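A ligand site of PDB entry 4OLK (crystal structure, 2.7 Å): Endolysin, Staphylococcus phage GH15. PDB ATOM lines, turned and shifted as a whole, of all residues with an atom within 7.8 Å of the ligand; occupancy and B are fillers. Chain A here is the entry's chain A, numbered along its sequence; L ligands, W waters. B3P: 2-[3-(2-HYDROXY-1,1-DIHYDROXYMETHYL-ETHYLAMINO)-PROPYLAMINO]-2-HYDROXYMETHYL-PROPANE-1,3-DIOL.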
ATOM      1  N   GLN A  56      16.038  -8.309 -37.163  1.00  0.00           N
ATOM      2  CA  GLN A  56      15.024  -7.716 -36.329  1.00  0.00           C
ATOM      3  C   GLN A  56      13.972  -8.725 -35.903  1.00  0.00           C
ATOM      4  O   GLN A  56      13.975  -9.859 -36.336  1.00  0.00           O
ATOM      5  CB  GLN A  56      14.362  -6.566 -37.072  1.00  0.00           C
ATOM      6  CG  GLN A  56      15.298  -5.438 -37.430  1.00  0.00           C
ATOM      7  CD  GLN A  56      15.562  -4.521 -36.268  1.00  0.00           C
ATOM      8  OE1 GLN A  56      14.630  -4.045 -35.624  1.00  0.00           O
ATOM      9  NE2 GLN A  56      16.817  -4.269 -35.991  1.00  0.00           N
ATOM     10  N   CYS A  57      13.072  -8.289 -35.024  1.00  0.00           N
ATOM     11  CA  CYS A  57      12.035  -9.150 -34.490  1.00  0.00           C
ATOM     12  C   CYS A  57      11.070  -9.616 -35.556  1.00  0.00           C
ATOM     13  O   CYS A  57      10.676 -10.773 -35.597  1.00  0.00           O
ATOM     14  CB  CYS A  57      11.279  -8.431 -33.350  1.00  0.00           C
ATOM     15  SG  CYS A  57      10.686  -6.779 -33.712  1.00  0.00           S
ATOM     16  N   PHE A 110       3.427  -7.842 -29.062  1.00  0.00           N
ATOM     17  CA  PHE A 110       3.656  -6.983 -27.919  1.00  0.00           C
ATOM     18  C   PHE A 110       3.535  -5.522 -28.312  1.00  0.00           C
ATOM     19  O   PHE A 110       4.429  -4.978 -28.937  1.00  0.00           O
ATOM     20  CB  PHE A 110       5.065  -7.230 -27.360  1.00  0.00           C
ATOM     21  CG  PHE A 110       5.335  -8.661 -26.990  1.00  0.00           C
ATOM     22  CD1 PHE A 110       5.822  -9.551 -27.923  1.00  0.00           C
ATOM     23  CD2 PHE A 110       5.140  -9.104 -25.697  1.00  0.00           C
ATOM     24  CE1 PHE A 110       6.083 -10.844 -27.583  1.00  0.00           C
ATOM     25  CE2 PHE A 110       5.401 -10.397 -25.358  1.00  0.00           C
ATOM     26  CZ  PHE A 110       5.873 -11.273 -26.299  1.00  0.00           C
ATOM     27  N   SER A 112       2.236  -3.027 -25.927  1.00  0.00           N
ATOM     28  CA  SER A 112       2.096  -2.173 -24.764  1.00  0.00           C
ATOM     29  C   SER A 112       3.273  -2.327 -23.800  1.00  0.00           C
ATOM     30  O   SER A 112       4.258  -2.994 -24.122  1.00  0.00           O
ATOM     31  CB  SER A 112       0.772  -2.423 -24.039  1.00  0.00           C
ATOM     32  OG  SER A 112       0.887  -3.458 -23.105  1.00  0.00           O
ATOM     33  N   SER A 114       6.611  -1.212 -21.719  1.00  0.00           N
ATOM     34  CA  SER A 114       7.796  -0.452 -22.048  1.00  0.00           C
ATOM     35  C   SER A 114       8.443  -0.943 -23.316  1.00  0.00           C
ATOM     36  O   SER A 114       9.612  -0.688 -23.538  1.00  0.00           O
ATOM     37  CB  SER A 114       8.807  -0.480 -20.912  1.00  0.00           C
ATOM     38  OG  SER A 114       8.413   0.342 -19.844  1.00  0.00           O
ATOM     39  N   TYR A 115       7.688  -1.657 -24.139  1.00  0.00           N
ATOM     40  CA  TYR A 115       8.233  -2.134 -25.398  1.00  0.00           C
ATOM     41  C   TYR A 115       8.365  -1.004 -26.407  1.00  0.00           C
ATOM     42  O   TYR A 115       7.817   0.068 -26.215  1.00  0.00           O
ATOM     43  CB  TYR A 115       7.390  -3.281 -25.968  1.00  0.00           C
ATOM     44  CG  TYR A 115       7.769  -4.653 -25.473  1.00  0.00           C
ATOM     45  CD1 TYR A 115       8.870  -5.316 -25.984  1.00  0.00           C
ATOM     46  CD2 TYR A 115       7.010  -5.294 -24.503  1.00  0.00           C
ATOM     47  CE1 TYR A 115       9.214  -6.565 -25.535  1.00  0.00           C
ATOM     48  CE2 TYR A 115       7.350  -6.551 -24.058  1.00  0.00           C
ATOM     49  CZ  TYR A 115       8.449  -7.180 -24.581  1.00  0.00           C
ATOM     50  OH  TYR A 115       8.782  -8.421 -24.133  1.00  0.00           O
ATOM     51  N   GLN A 116       9.104  -1.263 -27.476  1.00  0.00           N
ATOM     52  CA  GLN A 116       9.210  -0.338 -28.595  1.00  0.00           C
ATOM     53  C   GLN A 116       7.825   0.071 -29.036  1.00  0.00           C
ATOM     54  O   GLN A 116       6.860  -0.669 -28.892  1.00  0.00           O
ATOM     55  CB  GLN A 116       9.929  -0.990 -29.770  1.00  0.00           C
ATOM     56  CG  GLN A 116      11.287  -1.529 -29.459  1.00  0.00           C
ATOM     57  CD  GLN A 116      11.820  -2.426 -30.538  1.00  0.00           C
ATOM     58  OE1 GLN A 116      12.998  -2.385 -30.868  1.00  0.00           O
ATOM     59  NE2 GLN A 116      10.962  -3.255 -31.106  1.00  0.00           N
ATOM     60  N   GLN A 117       7.728   1.265 -29.593  1.00  0.00           N
ATOM     61  CA  GLN A 117       6.461   1.807 -30.022  1.00  0.00           C
ATOM     62  C   GLN A 117       5.978   1.061 -31.262  1.00  0.00           C
ATOM     63  O   GLN A 117       4.788   1.015 -31.534  1.00  0.00           O
ATOM     64  CB  GLN A 117       6.615   3.294 -30.309  1.00  0.00           C
ATOM     65  CG  GLN A 117       5.335   3.994 -30.619  1.00  0.00           C
ATOM     66  CD  GLN A 117       4.324   3.850 -29.520  1.00  0.00           C
ATOM     67  OE1 GLN A 117       4.677   3.844 -28.347  1.00  0.00           O
ATOM     68  NE2 GLN A 117       3.061   3.725 -29.896  1.00  0.00           N
ATOM     69  N   TRP A 118       6.917   0.476 -31.992  1.00  0.00           N
ATOM     70  CA  TRP A 118       6.590  -0.304 -33.172  1.00  0.00           C
ATOM     71  C   TRP A 118       6.458  -1.780 -32.858  1.00  0.00           C
ATOM     72  O   TRP A 118       6.234  -2.585 -33.742  1.00  0.00           O
ATOM     73  CB  TRP A 118       7.619  -0.070 -34.288  1.00  0.00           C
ATOM     74  CG  TRP A 118       9.034  -0.213 -33.871  1.00  0.00           C
ATOM     75  CD1 TRP A 118       9.796  -1.328 -33.955  1.00  0.00           C
ATOM     76  CD2 TRP A 118       9.874   0.805 -33.342  1.00  0.00           C
ATOM     77  NE1 TRP A 118      11.057  -1.072 -33.492  1.00  0.00           N
ATOM     78  CE2 TRP A 118      11.137   0.236 -33.107  1.00  0.00           C
ATOM     79  CE3 TRP A 118       9.684   2.152 -33.023  1.00  0.00           C
ATOM     80  CZ2 TRP A 118      12.194   0.946 -32.577  1.00  0.00           C
ATOM     81  CZ3 TRP A 118      10.735   2.855 -32.498  1.00  0.00           C
ATOM     82  CH2 TRP A 118      11.977   2.261 -32.288  1.00  0.00           C
ATOM     83  N   GLY A 119       6.609  -2.111 -31.592  1.00  0.00           N
ATOM     84  CA  GLY A 119       6.282  -3.439 -31.116  1.00  0.00           C
ATOM     85  C   GLY A 119       7.353  -4.506 -31.192  1.00  0.00           C
ATOM     86  O   GLY A 119       8.330  -4.402 -31.921  1.00  0.00           O
ATOM     87  N   HIS A 120       7.142  -5.546 -30.392  1.00  0.00           N
ATOM     88  CA  HIS A 120       7.939  -6.760 -30.454  1.00  0.00           C
ATOM     89  C   HIS A 120       7.050  -7.911 -30.859  1.00  0.00           C
ATOM     90  O   HIS A 120       5.842  -7.897 -30.638  1.00  0.00           O
ATOM     91  CB  HIS A 120       8.577  -7.051 -29.095  1.00  0.00           C
ATOM     92  CG  HIS A 120       9.472  -8.261 -29.104  1.00  0.00           C
ATOM     93  ND1 HIS A 120      10.578  -8.352 -29.916  1.00  0.00           N
ATOM     94  CD2 HIS A 120       9.411  -9.416 -28.413  1.00  0.00           C
ATOM     95  CE1 HIS A 120      11.159  -9.514 -29.716  1.00  0.00           C
ATOM     96  NE2 HIS A 120      10.472 -10.186 -28.811  1.00  0.00           N
ATOM     97  N   ILE A 121       7.662  -8.928 -31.453  1.00  0.00           N
ATOM     98  CA  ILE A 121       6.911 -10.031 -31.990  1.00  0.00           C
ATOM     99  C   ILE A 121       7.723 -11.319 -31.939  1.00  0.00           C
ATOM    100  O   ILE A 121       8.952 -11.288 -31.945  1.00  0.00           O
ATOM    101  CB  ILE A 121       6.454  -9.720 -33.429  1.00  0.00           C
ATOM    102  CG1 ILE A 121       5.234 -10.567 -33.806  1.00  0.00           C
ATOM    103  CG2 ILE A 121       7.602  -9.828 -34.407  1.00  0.00           C
ATOM    104  CD1 ILE A 121       4.433  -9.986 -34.922  1.00  0.00           C
ATOM    105  N   GLU A 137      11.979 -15.796 -30.446  1.00  0.00           N
ATOM    106  CA  GLU A 137      11.957 -14.419 -30.925  1.00  0.00           C
ATOM    107  C   GLU A 137      13.325 -13.994 -31.417  1.00  0.00           C
ATOM    108  O   GLU A 137      14.322 -14.644 -31.156  1.00  0.00           O
ATOM    109  CB  GLU A 137      11.538 -13.518 -29.788  1.00  0.00           C
ATOM    110  CG  GLU A 137      12.312 -13.815 -28.534  1.00  0.00           C
ATOM    111  CD  GLU A 137      11.962 -12.922 -27.384  1.00  0.00           C
ATOM    112  OE1 GLU A 137      10.990 -12.168 -27.494  1.00  0.00           O
ATOM    113  OE2 GLU A 137      12.678 -12.984 -26.365  1.00  0.00           O
ATOM    114  N   GLN A 138      13.348 -12.878 -32.137  1.00  0.00           N
ATOM    115  CA  GLN A 138      14.593 -12.233 -32.527  1.00  0.00           C
ATOM    116  C   GLN A 138      14.600 -10.813 -31.975  1.00  0.00           C
ATOM    117  O   GLN A 138      13.557 -10.200 -31.813  1.00  0.00           O
ATOM    118  CB  GLN A 138      14.759 -12.201 -34.040  1.00  0.00           C
ATOM    119  CG  GLN A 138      15.408 -13.446 -34.612  1.00  0.00           C
ATOM    120  CD  GLN A 138      15.851 -13.272 -36.044  1.00  0.00           C
ATOM    121  OE1 GLN A 138      16.676 -14.031 -36.538  1.00  0.00           O
ATOM    122  NE2 GLN A 138      15.318 -12.275 -36.719  1.00  0.00           N
ATOM    123  N   ASN A 139      15.798 -10.318 -31.683  1.00  0.00           N
ATOM    124  CA  ASN A 139      16.022  -8.919 -31.309  1.00  0.00           C
ATOM    125  C   ASN A 139      15.354  -8.444 -30.015  1.00  0.00           C
ATOM    126  O   ASN A 139      14.795  -7.361 -29.966  1.00  0.00           O
ATOM    127  CB  ASN A 139      15.637  -8.001 -32.462  1.00  0.00           C
ATOM    128  CG  ASN A 139      16.250  -6.635 -32.353  1.00  0.00           C
ATOM    129  OD1 ASN A 139      17.416  -6.494 -31.998  1.00  0.00           O
ATOM    130  ND2 ASN A 139      15.466  -5.619 -32.632  1.00  0.00           N
ATOM    131  N   TRP A 140      15.448  -9.240 -28.959  1.00  0.00           N
ATOM    132  CA  TRP A 140      14.991  -8.793 -27.672  1.00  0.00           C
ATOM    133  C   TRP A 140      16.108  -8.006 -27.021  1.00  0.00           C
ATOM    134  O   TRP A 140      15.873  -7.216 -26.123  1.00  0.00           O
ATOM    135  CB  TRP A 140      14.580  -9.972 -26.789  1.00  0.00           C
ATOM    136  CG  TRP A 140      13.608  -9.625 -25.706  1.00  0.00           C
ATOM    137  CD1 TRP A 140      12.260  -9.457 -25.834  1.00  0.00           C
ATOM    138  CD2 TRP A 140      13.901  -9.411 -24.319  1.00  0.00           C
ATOM    139  NE1 TRP A 140      11.698  -9.161 -24.626  1.00  0.00           N
ATOM    140  CE2 TRP A 140      12.676  -9.127 -23.677  1.00  0.00           C
ATOM    141  CE3 TRP A 140      15.062  -9.441 -23.553  1.00  0.00           C
ATOM    142  CZ2 TRP A 140      12.597  -8.866 -22.310  1.00  0.00           C
ATOM    143  CZ3 TRP A 140      14.978  -9.191 -22.207  1.00  0.00           C
ATOM    144  CH2 TRP A 140      13.758  -8.906 -21.594  1.00  0.00           C
ATOM    145  N   ASN A 141      17.335  -8.229 -27.481  1.00  0.00           N
ATOM    146  CA  ASN A 141      18.498  -7.503 -26.994  1.00  0.00           C
ATOM    147  C   ASN A 141      18.620  -6.125 -27.620  1.00  0.00           C
ATOM    148  O   ASN A 141      19.405  -5.296 -27.157  1.00  0.00           O
ATOM    149  CB  ASN A 141      19.789  -8.316 -27.192  1.00  0.00           C
ATOM    150  CG  ASN A 141      20.133  -8.535 -28.648  1.00  0.00           C
ATOM    151  OD1 ASN A 141      19.323  -8.310 -29.543  1.00  0.00           O
ATOM    152  ND2 ASN A 141      21.345  -8.992 -28.891  1.00  0.00           N
ATOM    153  N   GLY A 142      17.849  -5.891 -28.657  1.00  0.00           N
ATOM    154  CA  GLY A 142      17.843  -4.619 -29.351  1.00  0.00           C
ATOM    155  C   GLY A 142      19.022  -4.447 -30.286  1.00  0.00           C
ATOM    156  O   GLY A 142      19.216  -3.379 -30.850  1.00  0.00           O
ATOM    157  N   TYR A 143      19.803  -5.508 -30.462  1.00  0.00           N
ATOM    158  CA  TYR A 143      21.038  -5.400 -31.209  1.00  0.00           C
ATOM    159  C   TYR A 143      20.993  -6.152 -32.542  1.00  0.00           C
ATOM    160  O   TYR A 143      21.883  -6.014 -33.353  1.00  0.00           O
ATOM    161  CB  TYR A 143      22.217  -5.846 -30.346  1.00  0.00           C
ATOM    162  CG  TYR A 143      23.519  -5.188 -30.727  1.00  0.00           C
ATOM    163  CD1 TYR A 143      23.549  -3.911 -31.264  1.00  0.00           C
ATOM    164  CD2 TYR A 143      24.729  -5.853 -30.563  1.00  0.00           C
ATOM    165  CE1 TYR A 143      24.729  -3.320 -31.610  1.00  0.00           C
ATOM    166  CE2 TYR A 143      25.909  -5.262 -30.909  1.00  0.00           C
ATOM    167  CZ  TYR A 143      25.905  -3.996 -31.438  1.00  0.00           C
ATOM    168  OH  TYR A 143      27.085  -3.404 -31.784  1.00  0.00           O
ATOM    169  N   ALA A 144      19.942  -6.938 -32.724  1.00  0.00           N
ATOM    170  CA  ALA A 144      19.636  -7.574 -34.019  1.00  0.00           C
ATOM    171  C   ALA A 144      20.689  -8.516 -34.580  1.00  0.00           C
ATOM    172  O   ALA A 144      20.859  -8.597 -35.791  1.00  0.00           O
ATOM    173  CB  ALA A 144      19.257  -6.518 -35.038  1.00  0.00           C
ATOM    174  N   ARG A 151      12.754 -17.641 -24.943  1.00  0.00           N
ATOM    175  CA  ARG A 151      12.638 -16.872 -23.725  1.00  0.00           C
ATOM    176  C   ARG A 151      11.329 -17.227 -23.057  1.00  0.00           C
ATOM    177  O   ARG A 151      10.346 -17.507 -23.734  1.00  0.00           O
ATOM    178  CB  ARG A 151      12.681 -15.375 -24.031  1.00  0.00           C
ATOM    179  CG  ARG A 151      12.564 -14.491 -22.809  1.00  0.00           C
ATOM    180  CD  ARG A 151      12.606 -13.017 -23.164  1.00  0.00           C
ATOM    181  NE  ARG A 151      11.495 -12.625 -24.024  1.00  0.00           N
ATOM    182  CZ  ARG A 151      10.305 -12.257 -23.584  1.00  0.00           C
ATOM    183  NH1 ARG A 151      10.049 -12.243 -22.285  1.00  0.00           N
ATOM    184  NH2 ARG A 151       9.366 -11.911 -24.448  1.00  0.00           N
HETATM  185  C1  B3P L   1      13.769  -5.806 -23.539  1.00  0.00           C
HETATM  186  C2  B3P L   1      13.063  -5.290 -24.749  1.00  0.00           C
HETATM  187  C3  B3P L   1      14.763  -4.797 -22.926  1.00  0.00           C
HETATM  188  N1  B3P L   1      15.263  -3.878 -23.916  1.00  0.00           N
HETATM  189  C4  B3P L   1      16.713  -3.749 -23.823  1.00  0.00           C
HETATM  190  C5  B3P L   1      17.182  -3.681 -22.358  1.00  0.00           C
HETATM  191  C6  B3P L   1      17.141  -2.463 -24.549  1.00  0.00           C
HETATM  192  C7  B3P L   1      17.367  -4.918 -24.531  1.00  0.00           C
HETATM  193  N2  B3P L   1      13.904  -5.451 -26.000  1.00  0.00           N
HETATM  194  C8  B3P L   1      13.296  -4.700 -27.111  1.00  0.00           C
HETATM  195  C9  B3P L   1      14.335  -4.504 -28.237  1.00  0.00           C
HETATM  196  C10 B3P L   1      12.832  -3.315 -26.629  1.00  0.00           C
HETATM  197  C11 B3P L   1      12.110  -5.479 -27.705  1.00  0.00           C
HETATM  198  O1  B3P L   1      15.093  -3.322 -27.978  1.00  0.00           O
HETATM  199  O2  B3P L   1      11.394  -3.212 -26.622  1.00  0.00           O
HETATM  200  O3  B3P L   1      12.522  -6.204 -28.826  1.00  0.00           O
HETATM  201  O4  B3P L   1      17.264  -2.340 -21.944  1.00  0.00           O
HETATM  202  O5  B3P L   1      17.163  -2.743 -25.960  1.00  0.00           O
HETATM  203  O6  B3P L   1      18.337  -5.512 -23.717  1.00  0.00           O
HETATM  204  O   HOH W   1      18.378  -1.227 -27.777  1.00  0.00           O
HETATM  205  O   HOH W   2      16.080  -1.511 -29.542  1.00  0.00           O
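O of Trp 140 is in hydrogen-bond range of N2 of the ligand, 2.6 Å away.
An oxygen (O3) of the ligand sits at hydrogen-bond distance from the backbone carbonyl oxygen (O) of Asn 139, at 2.8 Å.
A ring nitrogen (ND1) of His 120 lies within hydrogen-bond range of an oxygen (O3) of the ligand, 3.1 Å away.
N of Gln 116 lies within hydrogen-bond range of O2 of the ligand (3.1 Å).
NE1 of Trp 140 sits at hydrogen-bond distance from OH of Tyr 115 (3.0 Å).
N of Tyr 143 lies within hydrogen-bond range of OD1 of Asn 139.
The side-chain amide oxygen (OD1) of Asn 141 is in hydrogen-bond range of the backbone NH (N) of Tyr 143, at 3.0 Å.
The backbone carbonyl oxygen (O) of His 120 is in hydrogen-bond range of the backbone NH (N) of Phe 110 (2.9 Å).
The side-chain amide nitrogen (NE2) of Gln 116 lies close to the indole nitrogen (NE1) of Trp 118 (3.2 Å).
ND2 of Asn 139 lies within hydrogen-bond range of OE1 of Gln 56 (3.5 Å).
NE2 of Gln 116 lies within hydrogen-bond range of O of Gly 119, 3.0 Å away.
The backbone NH (N) of Gly 142 sits close to the side-chain amide oxygen (OD1) of Asn 139, 3.4 Å away.
Tyr 115 touches the ligand (CD1 to O2, 3.3 Å).
O of Asn 141 touches C7 of the ligand, at 3.3 Å.
CA of Gly 142 touches O1 of the ligand, 3.3 Å away.
Hydrophobic or aromatic side chains within 4 Å of the ligand: Tyr 115, His 120 and Trp 140.
Of the 21 residues printed, 7 come within 4 Å of the ligand.
The nearest printed residue that does not touch the ligand is Ser 114 (4.4 Å).
Water W2 bridges an oxygen (O1) of the ligand and the side-chain amide oxygen (OE1) of Gln 116.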
